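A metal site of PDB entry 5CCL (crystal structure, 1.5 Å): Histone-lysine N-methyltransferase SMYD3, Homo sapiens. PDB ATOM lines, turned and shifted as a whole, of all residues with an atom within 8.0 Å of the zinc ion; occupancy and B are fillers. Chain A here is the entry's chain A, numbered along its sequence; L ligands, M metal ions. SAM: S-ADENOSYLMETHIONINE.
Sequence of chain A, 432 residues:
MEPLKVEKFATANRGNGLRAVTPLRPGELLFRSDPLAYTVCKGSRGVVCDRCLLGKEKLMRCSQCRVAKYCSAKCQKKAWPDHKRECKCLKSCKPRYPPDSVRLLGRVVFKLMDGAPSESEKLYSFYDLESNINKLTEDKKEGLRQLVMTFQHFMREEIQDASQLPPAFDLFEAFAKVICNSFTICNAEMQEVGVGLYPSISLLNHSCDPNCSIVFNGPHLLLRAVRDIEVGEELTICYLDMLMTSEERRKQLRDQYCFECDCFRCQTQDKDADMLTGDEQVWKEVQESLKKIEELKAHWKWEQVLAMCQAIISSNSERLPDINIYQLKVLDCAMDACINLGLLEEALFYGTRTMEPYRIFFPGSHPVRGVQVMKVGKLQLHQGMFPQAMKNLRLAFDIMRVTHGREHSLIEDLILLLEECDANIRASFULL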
ATOM      1  N   HIS A 206      13.001  -6.149  17.748  1.00  0.00           N
ATOM      2  CA  HIS A 206      14.302  -6.009  18.398  1.00  0.00           C
ATOM      3  C   HIS A 206      15.277  -5.202  17.557  1.00  0.00           C
ATOM      4  O   HIS A 206      15.322  -5.370  16.315  1.00  0.00           O
ATOM      5  CB  HIS A 206      14.899  -7.392  18.608  1.00  0.00           C
ATOM      6  CG  HIS A 206      16.338  -7.404  18.967  1.00  0.00           C
ATOM      7  ND1 HIS A 206      16.794  -7.196  20.251  1.00  0.00           N
ATOM      8  CD2 HIS A 206      17.441  -7.502  18.174  1.00  0.00           C
ATOM      9  CE1 HIS A 206      18.110  -7.191  20.229  1.00  0.00           C
ATOM     10  NE2 HIS A 206      18.526  -7.360  18.990  1.00  0.00           N
ATOM     11  N   SER A 207      16.137  -4.473  18.247  1.00  0.00           N
ATOM     12  CA  SER A 207      17.376  -4.012  17.674  1.00  0.00           C
ATOM     13  C   SER A 207      18.454  -4.045  18.740  1.00  0.00           C
ATOM     14  O   SER A 207      18.179  -3.771  19.897  1.00  0.00           O
ATOM     15  CB  SER A 207      17.241  -2.564  17.147  1.00  0.00           C
ATOM     16  OG  SER A 207      18.512  -2.129  16.652  1.00  0.00           O
ATOM     17  N   CYS A 208      19.696  -4.268  18.313  1.00  0.00           N
ATOM     18  CA  CYS A 208      20.842  -4.174  19.234  1.00  0.00           C
ATOM     19  C   CYS A 208      21.233  -2.687  19.442  1.00  0.00           C
ATOM     20  O   CYS A 208      22.126  -2.418  20.243  1.00  0.00           O
ATOM     21  CB  CYS A 208      22.049  -5.025  18.726  1.00  0.00           C
ATOM     22  SG  CYS A 208      21.630  -6.768  18.321  1.00  0.00           S
ATOM     23  N   ASP A 209      20.597  -1.769  18.686  1.00  0.00           N
ATOM     24  CA  ASP A 209      20.762  -0.295  18.832  1.00  0.00           C
ATOM     25  C   ASP A 209      19.378   0.342  18.715  1.00  0.00           C
ATOM     26  O   ASP A 209      19.012   0.932  17.713  1.00  0.00           O
ATOM     27  CB  ASP A 209      21.737   0.252  17.832  1.00  0.00           C
ATOM     28  CG  ASP A 209      21.873   1.762  17.920  1.00  0.00           C
ATOM     29  OD1 ASP A 209      21.488   2.383  18.914  1.00  0.00           O
ATOM     30  OD2 ASP A 209      22.350   2.298  16.909  1.00  0.00           O
ATOM     31  N   CYS A 238      15.710  -3.350  22.759  1.00  0.00           N
ATOM     32  CA  CYS A 238      16.722  -4.407  22.738  1.00  0.00           C
ATOM     33  C   CYS A 238      16.242  -5.513  23.629  1.00  0.00           C
ATOM     34  O   CYS A 238      15.997  -5.314  24.823  1.00  0.00           O
ATOM     35  CB  CYS A 238      18.050  -3.858  23.217  1.00  0.00           C
ATOM     36  SG  CYS A 238      19.388  -5.055  23.059  1.00  0.00           S
ATOM     37  N   LEU A 240      17.899  -7.961  24.657  1.00  0.00           N
ATOM     38  CA  LEU A 240      19.060  -8.607  25.245  1.00  0.00           C
ATOM     39  C   LEU A 240      19.878  -7.758  26.171  1.00  0.00           C
ATOM     40  O   LEU A 240      19.907  -6.547  26.011  1.00  0.00           O
ATOM     41  CB  LEU A 240      20.018  -9.060  24.127  1.00  0.00           C
ATOM     42  CG  LEU A 240      19.449  -9.888  23.002  1.00  0.00           C
ATOM     43  CD1 LEU A 240      20.517 -10.152  21.959  1.00  0.00           C
ATOM     44  CD2 LEU A 240      18.928 -11.186  23.576  1.00  0.00           C
ATOM     45  N   SER A 246      28.487 -10.172  19.547  1.00  0.00           N
ATOM     46  CA  SER A 246      27.526 -10.424  18.481  1.00  0.00           C
ATOM     47  C   SER A 246      27.248 -11.930  18.309  1.00  0.00           C
ATOM     48  O   SER A 246      26.103 -12.306  17.997  1.00  0.00           O
ATOM     49  CB  SER A 246      27.894  -9.720  17.167  1.00  0.00           C
ATOM     50  OG  SER A 246      29.080 -10.292  16.640  1.00  0.00           O
ATOM     51  N   ARG A 249      24.824 -12.780  21.070  1.00  0.00           N
ATOM     52  CA  ARG A 249      23.527 -12.266  20.727  1.00  0.00           C
ATOM     53  C   ARG A 249      22.856 -13.128  19.657  1.00  0.00           C
ATOM     54  O   ARG A 249      21.651 -13.448  19.735  1.00  0.00           O
ATOM     55  CB  ARG A 249      23.598 -10.814  20.284  1.00  0.00           C
ATOM     56  CG  ARG A 249      24.108  -9.855  21.339  1.00  0.00           C
ATOM     57  CD  ARG A 249      23.820  -8.370  21.031  1.00  0.00           C
ATOM     58  NE  ARG A 249      24.266  -7.916  19.717  1.00  0.00           N
ATOM     59  CZ  ARG A 249      25.479  -7.486  19.416  1.00  0.00           C
ATOM     60  NH1 ARG A 249      26.449  -7.500  20.324  1.00  0.00           N
ATOM     61  NH2 ARG A 249      25.716  -7.075  18.184  1.00  0.00           N
ATOM     62  N   ARG A 250      23.654 -13.548  18.701  1.00  0.00           N
ATOM     63  CA  ARG A 250      23.112 -14.379  17.614  1.00  0.00           C
ATOM     64  C   ARG A 250      22.530 -15.664  18.176  1.00  0.00           C
ATOM     65  O   ARG A 250      21.447 -16.134  17.768  1.00  0.00           O
ATOM     66  CB  ARG A 250      24.197 -14.637  16.570  1.00  0.00           C
ATOM     67  CG  ARG A 250      23.813 -15.652  15.486  1.00  0.00           C
ATOM     68  CD  ARG A 250      24.877 -15.777  14.431  1.00  0.00           C
ATOM     69  NE  ARG A 250      24.878 -14.586  13.654  1.00  0.00           N
ATOM     70  CZ  ARG A 250      25.803 -13.646  13.629  1.00  0.00           C
ATOM     71  NH1 ARG A 250      26.970 -13.767  14.289  1.00  0.00           N
ATOM     72  NH2 ARG A 250      25.548 -12.536  12.926  1.00  0.00           N
ATOM     73  N   LEU A 253      19.187 -14.874  20.064  1.00  0.00           N
ATOM     74  CA  LEU A 253      18.102 -14.464  19.156  1.00  0.00           C
ATOM     75  C   LEU A 253      17.611 -15.623  18.313  1.00  0.00           C
ATOM     76  O   LEU A 253      16.411 -15.737  18.057  1.00  0.00           O
ATOM     77  CB  LEU A 253      18.488 -13.265  18.331  1.00  0.00           C
ATOM     78  CG  LEU A 253      18.833 -11.989  19.125  1.00  0.00           C
ATOM     79  CD1 LEU A 253      19.360 -10.927  18.208  1.00  0.00           C
ATOM     80  CD2 LEU A 253      17.655 -11.469  19.929  1.00  0.00           C
ATOM     81  N   PHE A 259      15.134 -15.668  14.983  1.00  0.00           N
ATOM     82  CA  PHE A 259      15.507 -14.776  13.878  1.00  0.00           C
ATOM     83  C   PHE A 259      16.977 -14.466  13.831  1.00  0.00           C
ATOM     84  O   PHE A 259      17.694 -14.663  14.832  1.00  0.00           O
ATOM     85  CB  PHE A 259      14.672 -13.462  13.833  1.00  0.00           C
ATOM     86  CG  PHE A 259      15.025 -12.465  14.890  1.00  0.00           C
ATOM     87  CD1 PHE A 259      14.452 -12.515  16.152  1.00  0.00           C
ATOM     88  CD2 PHE A 259      15.912 -11.456  14.620  1.00  0.00           C
ATOM     89  CE1 PHE A 259      14.748 -11.589  17.127  1.00  0.00           C
ATOM     90  CE2 PHE A 259      16.261 -10.552  15.623  1.00  0.00           C
ATOM     91  CZ  PHE A 259      15.685 -10.612  16.865  1.00  0.00           C
ATOM     92  N   GLU A 260      17.377 -13.956  12.663  1.00  0.00           N
ATOM     93  CA  GLU A 260      18.734 -13.542  12.376  1.00  0.00           C
ATOM     94  C   GLU A 260      18.744 -12.009  12.363  1.00  0.00           C
ATOM     95  O   GLU A 260      18.018 -11.406  11.571  1.00  0.00           O
ATOM     96  CB  GLU A 260      19.142 -14.110  10.984  1.00  0.00           C
ATOM     97  CG  GLU A 260      18.719 -15.586  10.716  1.00  0.00           C
ATOM     98  CD  GLU A 260      19.365 -16.575  11.651  1.00  0.00           C
ATOM     99  OE1 GLU A 260      20.304 -16.131  12.348  1.00  0.00           O
ATOM    100  OE2 GLU A 260      18.993 -17.795  11.666  1.00  0.00           O
ATOM    101  N   CYS A 261      19.542 -11.384  13.252  1.00  0.00           N
ATOM    102  CA  CYS A 261      19.482  -9.925  13.387  1.00  0.00           C
ATOM    103  C   CYS A 261      20.298  -9.267  12.253  1.00  0.00           C
ATOM    104  O   CYS A 261      21.497  -9.578  12.044  1.00  0.00           O
ATOM    105  CB  CYS A 261      20.010  -9.460  14.739  1.00  0.00           C
ATOM    106  SG  CYS A 261      19.730  -7.702  14.991  1.00  0.00           S
ATOM    107  N   ASP A 262      19.661  -8.341  11.539  1.00  0.00           N
ATOM    108  CA  ASP A 262      20.328  -7.597  10.478  1.00  0.00           C
ATOM    109  C   ASP A 262      20.722  -6.190  10.881  1.00  0.00           C
ATOM    110  O   ASP A 262      20.970  -5.347   9.999  1.00  0.00           O
ATOM    111  CB  ASP A 262      19.427  -7.578   9.218  1.00  0.00           C
ATOM    112  CG  ASP A 262      18.181  -6.674   9.334  1.00  0.00           C
ATOM    113  OD1 ASP A 262      17.899  -6.145  10.442  1.00  0.00           O
ATOM    114  OD2 ASP A 262      17.435  -6.565   8.305  1.00  0.00           O
ATOM    115  N   CYS A 263      20.709  -5.870  12.174  1.00  0.00           N
ATOM    116  CA  CYS A 263      20.982  -4.504  12.567  1.00  0.00           C
ATOM    117  C   CYS A 263      22.448  -4.151  12.251  1.00  0.00           C
ATOM    118  O   CYS A 263      23.287  -5.025  12.017  1.00  0.00           O
ATOM    119  CB  CYS A 263      20.669  -4.240  14.013  1.00  0.00           C
ATOM    120  SG  CYS A 263      21.944  -4.658  15.216  1.00  0.00           S
ATOM    121  N   PHE A 264      22.733  -2.856  12.183  1.00  0.00           N
ATOM    122  CA  PHE A 264      24.072  -2.460  11.777  1.00  0.00           C
ATOM    123  C   PHE A 264      25.149  -2.888  12.746  1.00  0.00           C
ATOM    124  O   PHE A 264      26.284  -3.135  12.364  1.00  0.00           O
ATOM    125  CB  PHE A 264      24.073  -0.952  11.480  1.00  0.00           C
ATOM    126  CG  PHE A 264      25.208  -0.484  10.593  1.00  0.00           C
ATOM    127  CD1 PHE A 264      25.566  -1.168   9.438  1.00  0.00           C
ATOM    128  CD2 PHE A 264      25.882   0.669  10.923  1.00  0.00           C
ATOM    129  CE1 PHE A 264      26.577  -0.690   8.617  1.00  0.00           C
ATOM    130  CE2 PHE A 264      26.904   1.163  10.093  1.00  0.00           C
ATOM    131  CZ  PHE A 264      27.221   0.475   8.951  1.00  0.00           C
ATOM    132  N   ARG A 265      24.809  -2.963  14.026  1.00  0.00           N
ATOM    133  CA  ARG A 265      25.771  -3.496  14.990  1.00  0.00           C
ATOM    134  C   ARG A 265      26.176  -4.937  14.717  1.00  0.00           C
ATOM    135  O   ARG A 265      27.318  -5.286  14.808  1.00  0.00           O
ATOM    136  CB  ARG A 265      25.280  -3.398  16.427  1.00  0.00           C
ATOM    137  CG  ARG A 265      25.262  -1.983  16.962  1.00  0.00           C
ATOM    138  CD  ARG A 265      25.079  -1.970  18.460  1.00  0.00           C
ATOM    139  NE  ARG A 265      26.221  -2.581  19.084  1.00  0.00           N
ATOM    140  CZ  ARG A 265      26.225  -3.451  20.094  1.00  0.00           C
ATOM    141  NH1 ARG A 265      25.109  -3.753  20.770  1.00  0.00           N
ATOM    142  NH2 ARG A 265      27.355  -3.911  20.495  1.00  0.00           N
ATOM    143  N   CYS A 266      25.223  -5.757  14.329  1.00  0.00           N
ATOM    144  CA  CYS A 266      25.501  -7.132  13.989  1.00  0.00           C
ATOM    145  C   CYS A 266      26.275  -7.199  12.640  1.00  0.00           C
ATOM    146  O   CYS A 266      27.171  -7.983  12.499  1.00  0.00           O
ATOM    147  CB  CYS A 266      24.246  -7.975  13.987  1.00  0.00           C
ATOM    148  SG  CYS A 266      23.579  -8.146  15.672  1.00  0.00           S
ATOM    149  N   GLN A 267      25.941  -6.348  11.675  1.00  0.00           N
ATOM    150  CA  GLN A 267      26.658  -6.338  10.404  1.00  0.00           C
ATOM    151  C   GLN A 267      28.136  -5.942  10.585  1.00  0.00           C
ATOM    152  O   GLN A 267      29.010  -6.408   9.805  1.00  0.00           O
ATOM    153  CB  GLN A 267      25.996  -5.377   9.445  1.00  0.00           C
ATOM    154  CG  GLN A 267      24.603  -5.820   8.980  1.00  0.00           C
ATOM    155  CD  GLN A 267      24.002  -4.819   8.036  1.00  0.00           C
ATOM    156  OE1 GLN A 267      22.847  -4.462   8.144  1.00  0.00           O
ATOM    157  NE2 GLN A 267      24.806  -4.332   7.115  1.00  0.00           N
HETATM  158  N   SAM L   1       7.090  -9.294  14.940  1.00  0.00           N
HETATM  159  CA  SAM L   1       6.393  -9.749  16.161  1.00  0.00           C
HETATM  160  C   SAM L   1       4.949 -10.137  15.864  1.00  0.00           C
HETATM  161  O   SAM L   1       4.211 -10.435  16.838  1.00  0.00           O
HETATM  162  OXT SAM L   1       4.583 -10.150  14.661  1.00  0.00           O
HETATM  163  CB  SAM L   1       6.503  -8.769  17.323  1.00  0.00           C
HETATM  164  CG  SAM L   1       7.769  -8.958  18.222  1.00  0.00           C
HETATM  165  SD  SAM L   1       7.744 -10.479  19.090  1.00  0.00           S
HETATM  166  CE  SAM L   1       8.090 -10.137  20.720  1.00  0.00           C
HETATM  167  C5' SAM L   1       9.233 -11.277  18.694  1.00  0.00           C
HETATM  168  C4' SAM L   1       9.316 -11.902  17.304  1.00  0.00           C
HETATM  169  O4' SAM L   1       9.398 -10.885  16.282  1.00  0.00           O
HETATM  170  C3' SAM L   1      10.554 -12.734  17.073  1.00  0.00           C
HETATM  171  O3' SAM L   1      10.455 -14.036  17.623  1.00  0.00           O
HETATM  172  C2' SAM L   1      10.662 -12.676  15.588  1.00  0.00           C
HETATM  173  O2' SAM L   1       9.653 -13.497  14.933  1.00  0.00           O
HETATM  174  C1' SAM L   1      10.338 -11.230  15.265  1.00  0.00           C
HETATM  175  N9  SAM L   1      11.451 -10.261  15.391  1.00  0.00           N
HETATM  176  C8  SAM L   1      11.670  -9.371  16.407  1.00  0.00           C
HETATM  177  N7  SAM L   1      12.700  -8.561  16.086  1.00  0.00           N
HETATM  178  C5  SAM L   1      13.152  -8.953  14.841  1.00  0.00           C
HETATM  179  C6  SAM L   1      14.200  -8.481  13.987  1.00  0.00           C
HETATM  180  N6  SAM L   1      14.992  -7.471  14.347  1.00  0.00           N
HETATM  181  N1  SAM L   1      14.377  -9.116  12.803  1.00  0.00           N
HETATM  182  C2  SAM L   1      13.560 -10.137  12.486  1.00  0.00           C
HETATM  183  N3  SAM L   1      12.523 -10.623  13.200  1.00  0.00           N
HETATM  184  C4  SAM L   1      12.315 -10.035  14.392  1.00  0.00           C
HETATM  185 ZN    ZN M   1      21.679  -6.844  15.939  1.00  0.00          ZN
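The backbone NH (N) of His 206 lies within hydrogen-bond range of a nitrogen (N7) of the ligand (2.9 Å).
A nitrogen (N6) of the ligand lies within hydrogen-bond range of the backbone carbonyl oxygen (O) of His 206.
SG of Cys 263 lies close to N of Arg 265.
The side-chain sulfur of Cys 266 sits close to the guanidinium group of Arg 249.
A ring nitrogen (NE2) of His 206 is in hydrogen-bond range of the backbone NH (N) of Cys 208.
SG of Cys 208 sits close to NE of Arg 249 (3.2 Å).
The backbone carbonyl oxygen of Cys 208 is in hydrogen-bond range of the guanidinium group of Arg 265 (3.3 Å).
The zinc ion is bound by SG of Cys 263 (2.3 Å), SG of Cys 266 (2.3 Å), SG of Cys 261 (2.3 Å) and SG of Cys 208 (2.4 Å).
The zinc ion has four donor atoms within binding distance.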
